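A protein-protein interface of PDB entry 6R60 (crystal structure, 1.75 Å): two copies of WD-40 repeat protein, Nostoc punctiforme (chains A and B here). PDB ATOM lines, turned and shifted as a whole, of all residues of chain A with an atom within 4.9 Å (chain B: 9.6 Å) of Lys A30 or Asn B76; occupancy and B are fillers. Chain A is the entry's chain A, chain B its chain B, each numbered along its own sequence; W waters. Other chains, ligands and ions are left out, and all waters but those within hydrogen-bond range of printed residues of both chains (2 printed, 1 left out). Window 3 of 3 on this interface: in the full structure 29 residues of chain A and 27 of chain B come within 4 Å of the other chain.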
ATOM      1  N   ILE A  20      15.007  28.202  17.091  1.00  0.00           N
ATOM      2  CA  ILE A  20      15.376  28.174  15.655  1.00  0.00           C
ATOM      3  C   ILE A  20      15.210  26.742  15.147  1.00  0.00           C
ATOM      4  O   ILE A  20      15.717  25.835  15.765  1.00  0.00           O
ATOM      5  CB  ILE A  20      16.830  28.624  15.447  1.00  0.00           C
ATOM      6  CG1 ILE A  20      17.030  30.063  15.947  1.00  0.00           C
ATOM      7  CG2 ILE A  20      17.235  28.521  13.986  1.00  0.00           C
ATOM      8  CD1 ILE A  20      18.490  30.392  16.188  1.00  0.00           C
ATOM      9  N   ALA A  21      14.513  26.559  14.033  1.00  0.00           N
ATOM     10  CA  ALA A  21      14.345  25.232  13.416  1.00  0.00           C
ATOM     11  C   ALA A  21      15.116  25.195  12.124  1.00  0.00           C
ATOM     12  O   ALA A  21      15.159  26.188  11.357  1.00  0.00           O
ATOM     13  CB  ALA A  21      12.889  24.944  13.124  1.00  0.00           C
ATOM     14  N   SER A  22      15.719  24.046  11.854  1.00  0.00           N
ATOM     15  CA  SER A  22      16.354  23.860  10.582  1.00  0.00           C
ATOM     16  C   SER A  22      16.358  22.417  10.149  1.00  0.00           C
ATOM     17  O   SER A  22      16.637  21.537  10.950  1.00  0.00           O
ATOM     18  CB  SER A  22      17.781  24.374  10.582  1.00  0.00           C
ATOM     19  OG  SER A  22      18.164  24.423   9.223  1.00  0.00           O
ATOM     20  N   SER A  24      17.941  19.288   8.606  1.00  0.00           N
ATOM     21  CA  SER A  24      19.285  18.748   8.558  1.00  0.00           C
ATOM     22  C   SER A  24      19.471  17.825   7.364  1.00  0.00           C
ATOM     23  O   SER A  24      18.516  17.282   6.811  1.00  0.00           O
ATOM     24  CB  SER A  24      19.575  17.967   9.840  1.00  0.00           C
ATOM     25  OG  SER A  24      19.270  18.766  10.947  1.00  0.00           O
ATOM     26  N   ASP A  25      20.733  17.621   7.021  1.00  0.00           N
ATOM     27  CA  ASP A  25      21.122  16.676   5.996  1.00  0.00           C
ATOM     28  C   ASP A  25      20.554  15.277   6.220  1.00  0.00           C
ATOM     29  O   ASP A  25      20.320  14.564   5.244  1.00  0.00           O
ATOM     30  CB  ASP A  25      22.656  16.565   5.930  1.00  0.00           C
ATOM     31  CG  ASP A  25      23.306  17.734   5.217  1.00  0.00           C
ATOM     32  OD1 ASP A  25      22.583  18.672   4.823  1.00  0.00           O
ATOM     33  OD2 ASP A  25      24.546  17.706   5.035  1.00  0.00           O
ATOM     34  N   ASP A  26      20.358  14.875   7.487  1.00  0.00           N
ATOM     35  CA  ASP A  26      19.869  13.500   7.807  1.00  0.00           C
ATOM     36  C   ASP A  26      18.333  13.342   7.816  1.00  0.00           C
ATOM     37  O   ASP A  26      17.821  12.354   8.327  1.00  0.00           O
ATOM     38  CB  ASP A  26      20.450  12.991   9.148  1.00  0.00           C
ATOM     39  CG  ASP A  26      20.027  13.832  10.349  1.00  0.00           C
ATOM     40  OD1 ASP A  26      19.171  14.735  10.199  1.00  0.00           O
ATOM     41  OD2 ASP A  26      20.570  13.610  11.465  1.00  0.00           O
ATOM     42  N   THR A  28      16.071  14.970   9.448  1.00  0.00           N
ATOM     43  CA  THR A  28      15.439  15.440  10.655  1.00  0.00           C
ATOM     44  C   THR A  28      15.320  16.987  10.567  1.00  0.00           C
ATOM     45  O   THR A  28      15.946  17.631   9.700  1.00  0.00           O
ATOM     46  CB  THR A  28      16.308  15.085  11.913  1.00  0.00           C
ATOM     47  OG1 THR A  28      17.574  15.771  11.856  1.00  0.00           O
ATOM     48  CG2 THR A  28      16.543  13.576  12.021  1.00  0.00           C
ATOM     49  N   VAL A  29      14.541  17.555  11.480  1.00  0.00           N
ATOM     50  CA  VAL A  29      14.543  18.981  11.718  1.00  0.00           C
ATOM     51  C   VAL A  29      15.075  19.154  13.139  1.00  0.00           C
ATOM     52  O   VAL A  29      14.634  18.498  14.060  1.00  0.00           O
ATOM     53  CB  VAL A  29      13.128  19.570  11.600  1.00  0.00           C
ATOM     54  CG1 VAL A  29      13.069  21.002  12.047  1.00  0.00           C
ATOM     55  CG2 VAL A  29      12.639  19.402  10.166  1.00  0.00           C
ATOM     56  N   LYS A  30      16.053  20.021  13.294  1.00  0.00           N
ATOM     57  CA  LYS A  30      16.618  20.292  14.601  1.00  0.00           C
ATOM     58  C   LYS A  30      16.050  21.611  15.121  1.00  0.00           C
ATOM     59  O   LYS A  30      15.893  22.552  14.348  1.00  0.00           O
ATOM     60  CB  LYS A  30      18.135  20.451  14.481  1.00  0.00           C
ATOM     61  CG  LYS A  30      18.834  19.300  13.798  1.00  0.00           C
ATOM     62  CD  LYS A  30      19.643  18.459  14.746  1.00  0.00           C
ATOM     63  CE  LYS A  30      20.431  17.414  13.984  1.00  0.00           C
ATOM     64  NZ  LYS A  30      21.548  16.896  14.814  1.00  0.00           N
ATOM     65  N   LEU A  31      15.803  21.670  16.438  1.00  0.00           N
ATOM     66  CA  LEU A  31      15.448  22.911  17.145  1.00  0.00           C
ATOM     67  C   LEU A  31      16.593  23.331  18.078  1.00  0.00           C
ATOM     68  O   LEU A  31      17.082  22.527  18.886  1.00  0.00           O
ATOM     69  CB  LEU A  31      14.146  22.688  17.925  1.00  0.00           C
ATOM     70  CG  LEU A  31      12.965  22.038  17.168  1.00  0.00           C
ATOM     71  CD1 LEU A  31      11.732  21.992  18.057  1.00  0.00           C
ATOM     72  CD2 LEU A  31      12.590  22.757  15.901  1.00  0.00           C
ATOM     73  N   TRP A  32      17.023  24.573  17.951  1.00  0.00           N
ATOM     74  CA  TRP A  32      18.137  25.095  18.708  1.00  0.00           C
ATOM     75  C   TRP A  32      17.585  26.259  19.509  1.00  0.00           C
ATOM     76  O   TRP A  32      16.607  26.885  19.082  1.00  0.00           O
ATOM     77  CB  TRP A  32      19.226  25.618  17.771  1.00  0.00           C
ATOM     78  CG  TRP A  32      19.540  24.741  16.495  1.00  0.00           C
ATOM     79  CD1 TRP A  32      19.071  24.910  15.214  1.00  0.00           C
ATOM     80  CD2 TRP A  32      20.449  23.666  16.456  1.00  0.00           C
ATOM     81  NE1 TRP A  32      19.610  23.953  14.376  1.00  0.00           N
ATOM     82  CE2 TRP A  32      20.469  23.173  15.122  1.00  0.00           C
ATOM     83  CE3 TRP A  32      21.216  23.034  17.427  1.00  0.00           C
ATOM     84  CZ2 TRP A  32      21.208  22.099  14.759  1.00  0.00           C
ATOM     85  CZ3 TRP A  32      21.958  21.956  17.064  1.00  0.00           C
ATOM     86  CH2 TRP A  32      21.943  21.481  15.737  1.00  0.00           C
ATOM     87  N   LEU A  38      21.343  22.448  21.291  1.00  0.00           N
ATOM     88  CA  LEU A  38      20.250  21.662  20.766  1.00  0.00           C
ATOM     89  C   LEU A  38      19.133  21.616  21.783  1.00  0.00           C
ATOM     90  O   LEU A  38      19.387  21.520  22.996  1.00  0.00           O
ATOM     91  CB  LEU A  38      20.724  20.237  20.464  1.00  0.00           C
ATOM     92  CG  LEU A  38      19.712  19.251  19.897  1.00  0.00           C
ATOM     93  CD1 LEU A  38      19.274  19.726  18.520  1.00  0.00           C
ATOM     94  CD2 LEU A  38      20.335  17.868  19.831  1.00  0.00           C
ATOM     95  N   GLN A  40      15.746  20.019  20.621  1.00  0.00           N
ATOM     96  CA  GLN A  40      14.982  18.833  20.214  1.00  0.00           C
ATOM     97  C   GLN A  40      15.302  18.465  18.784  1.00  0.00           C
ATOM     98  O   GLN A  40      15.754  19.297  17.997  1.00  0.00           O
ATOM     99  CB  GLN A  40      13.477  19.095  20.327  1.00  0.00           C
ATOM    100  CG  GLN A  40      12.623  17.843  20.229  1.00  0.00           C
ATOM    101  CD  GLN A  40      13.027  16.845  21.280  1.00  0.00           C
ATOM    102  OE1 GLN A  40      12.808  17.082  22.473  1.00  0.00           O
ATOM    103  NE2 GLN A  40      13.646  15.731  20.851  1.00  0.00           N
ATOM    104  N   THR A  41      15.093  17.189  18.452  1.00  0.00           N
ATOM    105  CA  THR A  41      15.244  16.698  17.098  1.00  0.00           C
ATOM    106  C   THR A  41      13.891  16.118  16.705  1.00  0.00           C
ATOM    107  O   THR A  41      13.323  15.322  17.454  1.00  0.00           O
ATOM    108  CB  THR A  41      16.303  15.606  17.057  1.00  0.00           C
ATOM    109  OG1 THR A  41      17.559  16.135  17.483  1.00  0.00           O
ATOM    110  CG2 THR A  41      16.477  15.007  15.669  1.00  0.00           C
ATOM    111  N   PHE B  54      19.900  33.378   8.222  1.00  0.00           N
ATOM    112  CA  PHE B  54      20.395  32.220   7.527  1.00  0.00           C
ATOM    113  C   PHE B  54      21.191  32.709   6.348  1.00  0.00           C
ATOM    114  O   PHE B  54      20.806  33.681   5.718  1.00  0.00           O
ATOM    115  CB  PHE B  54      19.191  31.406   7.093  1.00  0.00           C
ATOM    116  CG  PHE B  54      18.284  31.078   8.253  1.00  0.00           C
ATOM    117  CD1 PHE B  54      18.641  30.108   9.174  1.00  0.00           C
ATOM    118  CD2 PHE B  54      17.113  31.815   8.484  1.00  0.00           C
ATOM    119  CE1 PHE B  54      17.839  29.834  10.270  1.00  0.00           C
ATOM    120  CE2 PHE B  54      16.308  31.548   9.587  1.00  0.00           C
ATOM    121  CZ  PHE B  54      16.673  30.558  10.483  1.00  0.00           C
ATOM    122  N   GLY B  58      21.982  28.870   2.636  1.00  0.00           N
ATOM    123  CA  GLY B  58      21.135  28.135   3.535  1.00  0.00           C
ATOM    124  C   GLY B  58      21.874  27.217   4.486  1.00  0.00           C
ATOM    125  O   GLY B  58      21.215  26.541   5.271  1.00  0.00           O
ATOM    126  N   GLN B  59      23.220  27.228   4.469  1.00  0.00           N
ATOM    127  CA  GLN B  59      24.017  26.273   5.236  1.00  0.00           C
ATOM    128  C   GLN B  59      24.487  26.769   6.595  1.00  0.00           C
ATOM    129  O   GLN B  59      24.859  25.965   7.436  1.00  0.00           O
ATOM    130  CB  GLN B  59      25.222  25.784   4.409  1.00  0.00           C
ATOM    131  CG  GLN B  59      24.825  25.144   3.091  1.00  0.00           C
ATOM    132  CD  GLN B  59      23.750  24.074   3.255  1.00  0.00           C
ATOM    133  OE1 GLN B  59      23.891  23.133   4.059  1.00  0.00           O
ATOM    134  NE2 GLN B  59      22.654  24.222   2.504  1.00  0.00           N
ATOM    135  N   THR B  60      24.463  28.075   6.823  1.00  0.00           N
ATOM    136  CA  THR B  60      24.950  28.638   8.080  1.00  0.00           C
ATOM    137  C   THR B  60      23.826  29.416   8.743  1.00  0.00           C
ATOM    138  O   THR B  60      23.104  30.150   8.047  1.00  0.00           O
ATOM    139  CB  THR B  60      26.168  29.554   7.867  1.00  0.00           C
ATOM    140  OG1 THR B  60      27.210  28.826   7.224  1.00  0.00           O
ATOM    141  CG2 THR B  60      26.683  30.094   9.203  1.00  0.00           C
ATOM    142  N   ILE B  61      23.699  29.260  10.065  1.00  0.00           N
ATOM    143  CA  ILE B  61      22.751  30.029  10.876  1.00  0.00           C
ATOM    144  C   ILE B  61      23.554  30.957  11.731  1.00  0.00           C
ATOM    145  O   ILE B  61      24.564  30.562  12.300  1.00  0.00           O
ATOM    146  CB  ILE B  61      21.916  29.122  11.794  1.00  0.00           C
ATOM    147  CG1 ILE B  61      21.098  28.159  10.931  1.00  0.00           C
ATOM    148  CG2 ILE B  61      21.006  29.951  12.711  1.00  0.00           C
ATOM    149  CD1 ILE B  61      21.067  26.757  11.461  1.00  0.00           C
ATOM    150  N   TRP B  73      26.547  28.671  13.350  1.00  0.00           N
ATOM    151  CA  TRP B  73      26.593  27.226  13.341  1.00  0.00           C
ATOM    152  C   TRP B  73      26.025  26.671  12.025  1.00  0.00           C
ATOM    153  O   TRP B  73      25.336  27.364  11.249  1.00  0.00           O
ATOM    154  CB  TRP B  73      25.939  26.578  14.573  1.00  0.00           C
ATOM    155  CG  TRP B  73      24.487  26.747  14.797  1.00  0.00           C
ATOM    156  CD1 TRP B  73      23.481  25.892  14.411  1.00  0.00           C
ATOM    157  CD2 TRP B  73      23.875  27.721  15.658  1.00  0.00           C
ATOM    158  NE1 TRP B  73      22.265  26.326  14.907  1.00  0.00           N
ATOM    159  CE2 TRP B  73      22.492  27.460  15.669  1.00  0.00           C
ATOM    160  CE3 TRP B  73      24.363  28.849  16.357  1.00  0.00           C
ATOM    161  CZ2 TRP B  73      21.595  28.261  16.350  1.00  0.00           C
ATOM    162  CZ3 TRP B  73      23.468  29.629  17.057  1.00  0.00           C
ATOM    163  CH2 TRP B  73      22.101  29.322  17.062  1.00  0.00           C
ATOM    164  N   ASN B  74      26.442  25.475  11.699  1.00  0.00           N
ATOM    165  CA  ASN B  74      25.908  24.810  10.484  1.00  0.00           C
ATOM    166  C   ASN B  74      24.620  24.007  10.765  1.00  0.00           C
ATOM    167  O   ASN B  74      24.186  23.906  11.902  1.00  0.00           O
ATOM    168  CB  ASN B  74      27.009  24.021   9.799  1.00  0.00           C
ATOM    169  CG  ASN B  74      27.468  22.800  10.593  1.00  0.00           C
ATOM    170  OD1 ASN B  74      26.757  22.289  11.468  1.00  0.00           O
ATOM    171  ND2 ASN B  74      28.645  22.269  10.211  1.00  0.00           N
ATOM    172  N   ARG B  75      24.009  23.433   9.740  1.00  0.00           N
ATOM    173  CA  ARG B  75      22.745  22.708   9.948  1.00  0.00           C
ATOM    174  C   ARG B  75      22.810  21.437  10.795  1.00  0.00           C
ATOM    175  O   ARG B  75      21.778  20.952  11.312  1.00  0.00           O
ATOM    176  CB  ARG B  75      22.162  22.309   8.617  1.00  0.00           C
ATOM    177  CG  ARG B  75      21.712  23.499   7.841  1.00  0.00           C
ATOM    178  CD  ARG B  75      20.865  23.063   6.663  1.00  0.00           C
ATOM    179  NE  ARG B  75      20.145  24.200   6.123  1.00  0.00           N
ATOM    180  CZ  ARG B  75      18.947  24.146   5.544  1.00  0.00           C
ATOM    181  NH1 ARG B  75      18.287  22.995   5.376  1.00  0.00           N
ATOM    182  NH2 ARG B  75      18.418  25.277   5.106  1.00  0.00           N
ATOM    183  N   ASN B  76      24.016  20.892  10.908  1.00  0.00           N
ATOM    184  CA  ASN B  76      24.260  19.780  11.819  1.00  0.00           C
ATOM    185  C   ASN B  76      24.407  20.221  13.263  1.00  0.00           C
ATOM    186  O   ASN B  76      24.490  19.395  14.166  1.00  0.00           O
ATOM    187  CB  ASN B  76      25.548  19.059  11.451  1.00  0.00           C
ATOM    188  CG  ASN B  76      25.446  18.310  10.166  1.00  0.00           C
ATOM    189  OD1 ASN B  76      24.352  17.973   9.717  1.00  0.00           O
ATOM    190  ND2 ASN B  76      26.594  17.983   9.586  1.00  0.00           N
ATOM    191  N   GLY B  77      24.510  21.521  13.473  1.00  0.00           N
ATOM    192  CA  GLY B  77      24.690  22.078  14.805  1.00  0.00           C
ATOM    193  C   GLY B  77      26.115  22.379  15.218  1.00  0.00           C
ATOM    194  O   GLY B  77      26.340  22.776  16.375  1.00  0.00           O
ATOM    195  N   GLN B  78      27.074  22.211  14.315  1.00  0.00           N
ATOM    196  CA  GLN B  78      28.478  22.431  14.677  1.00  0.00           C
ATOM    197  C   GLN B  78      28.717  23.896  14.771  1.00  0.00           C
ATOM    198  O   GLN B  78      28.332  24.650  13.865  1.00  0.00           O
ATOM    199  CB  GLN B  78      29.428  21.827  13.648  1.00  0.00           C
ATOM    200  CG  GLN B  78      29.332  20.342  13.545  1.00  0.00           C
ATOM    201  CD  GLN B  78      30.162  19.770  12.426  1.00  0.00           C
ATOM    202  OE1 GLN B  78      31.374  19.582  12.547  1.00  0.00           O
ATOM    203  NE2 GLN B  78      29.492  19.433  11.346  1.00  0.00           N
ATOM    204  N   LEU B  79      29.295  24.326  15.901  1.00  0.00           N
ATOM    205  CA  LEU B  79      29.615  25.713  16.110  1.00  0.00           C
ATOM    206  C   LEU B  79      30.773  26.061  15.196  1.00  0.00           C
ATOM    207  O   LEU B  79      31.784  25.362  15.181  1.00  0.00           O
ATOM    208  CB  LEU B  79      29.990  25.979  17.573  1.00  0.00           C
ATOM    209  CG  LEU B  79      30.376  27.416  17.929  1.00  0.00           C
ATOM    210  CD1 LEU B  79      29.188  28.329  17.789  1.00  0.00           C
ATOM    211  CD2 LEU B  79      30.945  27.481  19.331  1.00  0.00           C
ATOM    212  N   LEU B  80      30.620  27.116  14.421  1.00  0.00           N
ATOM    213  CA  LEU B  80      31.640  27.526  13.488  1.00  0.00           C
ATOM    214  C   LEU B  80      32.468  28.692  14.013  1.00  0.00           C
ATOM    215  O   LEU B  80      33.669  28.715  13.829  1.00  0.00           O
ATOM    216  CB  LEU B  80      30.987  27.937  12.155  1.00  0.00           C
ATOM    217  CG  LEU B  80      30.196  26.812  11.478  1.00  0.00           C
ATOM    218  CD1 LEU B  80      29.481  27.295  10.221  1.00  0.00           C
ATOM    219  CD2 LEU B  80      31.092  25.627  11.171  1.00  0.00           C
HETATM  220  O   HOH W   1      22.157  16.954  11.473  1.00  0.00           O
HETATM  221  O   HOH W   2      22.630  15.600   9.305  1.00  0.00           O
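No position is printed for both chains.
Lys A30 touches one residue of chain B. Asn B76 touches just these residues of chain A: Lys A30 (3.9 Å) and Trp A32 (3.6 Å). No residue of chain B comes within 4 Å of Ala A21. Of the printed residues of chain B, Ile A20 touches Phe B54 (3.99 Å) and Trp B73 (3.8 Å). Of the printed residues of chain B, Ser A24 touches Arg B75 (3.3 Å). Of the printed residues of chain A, Arg B75 touches Ser A22, Ser A24 and Trp A32. Printed residues of chain B within 4 Å of Ser A22: Arg B75. Of the printed residues of chain B, Trp A32 touches Trp B73 (3.5 Å), Arg B75 (3.7 Å), Asn B76 (3.6 Å) and Gly B77 (3.0 Å). Gln A40 touches none of the printed residues of chain B. Leu B80 touches none of the printed residues of chain A.
CG2 of Ile A20 touches CE1 of Phe B54, at 3.99 Å. CD1 of Ile A20 touches CZ2 of Trp B73, 3.8 Å away. Ser A22 touches Arg B75. Lys A30 touches Asn B76 (NZ to O, 3.9 Å). Trp B73 touches Trp A32. Trp A32 touches Arg B75. CH2 of Trp A32 touches O of Asn B76 (3.6 Å). CA of Gly B77 touches CH2 of Trp A32 (3.0 Å).
The backbone carbonyl oxygen (O) of Ile A20 is in hydrogen-bond range of the backbone NH (N) of Trp A32, 2.8 Å away. The backbone NH (N) of Lys A30 sits at hydrogen-bond distance from the backbone carbonyl oxygen (O) of Ser A22. O of Gly B58 is in hydrogen-bond range of NE of Arg B75 (2.7 Å). The backbone NH (N) of Ile B61 lies within hydrogen-bond range of the backbone carbonyl oxygen (O) of Trp B73. N of Asn B76 is in hydrogen-bond range of OD1 of Asn B74, 3.1 Å away. OD1 of Asn B74 is in hydrogen-bond range of N of Gly B77 (3.1 Å).
Of the 13 printed residues of chain B, 5 touch a printed residue of chain A. Hydrophobic or aromatic side chains of chain B that line the printed part of chain A: Phe B54 and Trp B73. Hydrophobic or aromatic side chains of chain A that line the printed part of chain B: Ile A20 and Trp A32. Among the printed residues, 9 pairs touch across the chains. Among the printed residues, no Asp or Glu carboxylate lies within 4 Å of a Lys or Arg side-chain nitrogen of the other chain.
Water W2 lies within hydrogen-bond range of OD1 of Asn B76 (3.0 Å) and N of Asp A26 (3.0 Å). Water W1 lies within hydrogen-bond range of the side-chain amide oxygen of Asn B76 (3.0 Å), the side-chain amino group of Lys A30 (3.4 Å) and the side-chain hydroxyl of Ser A24 (3.4 Å).
The side-chain hydroxyl (OG) of Ser A24 is in hydrogen-bond range of the backbone carbonyl oxygen (O) of Arg B75.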
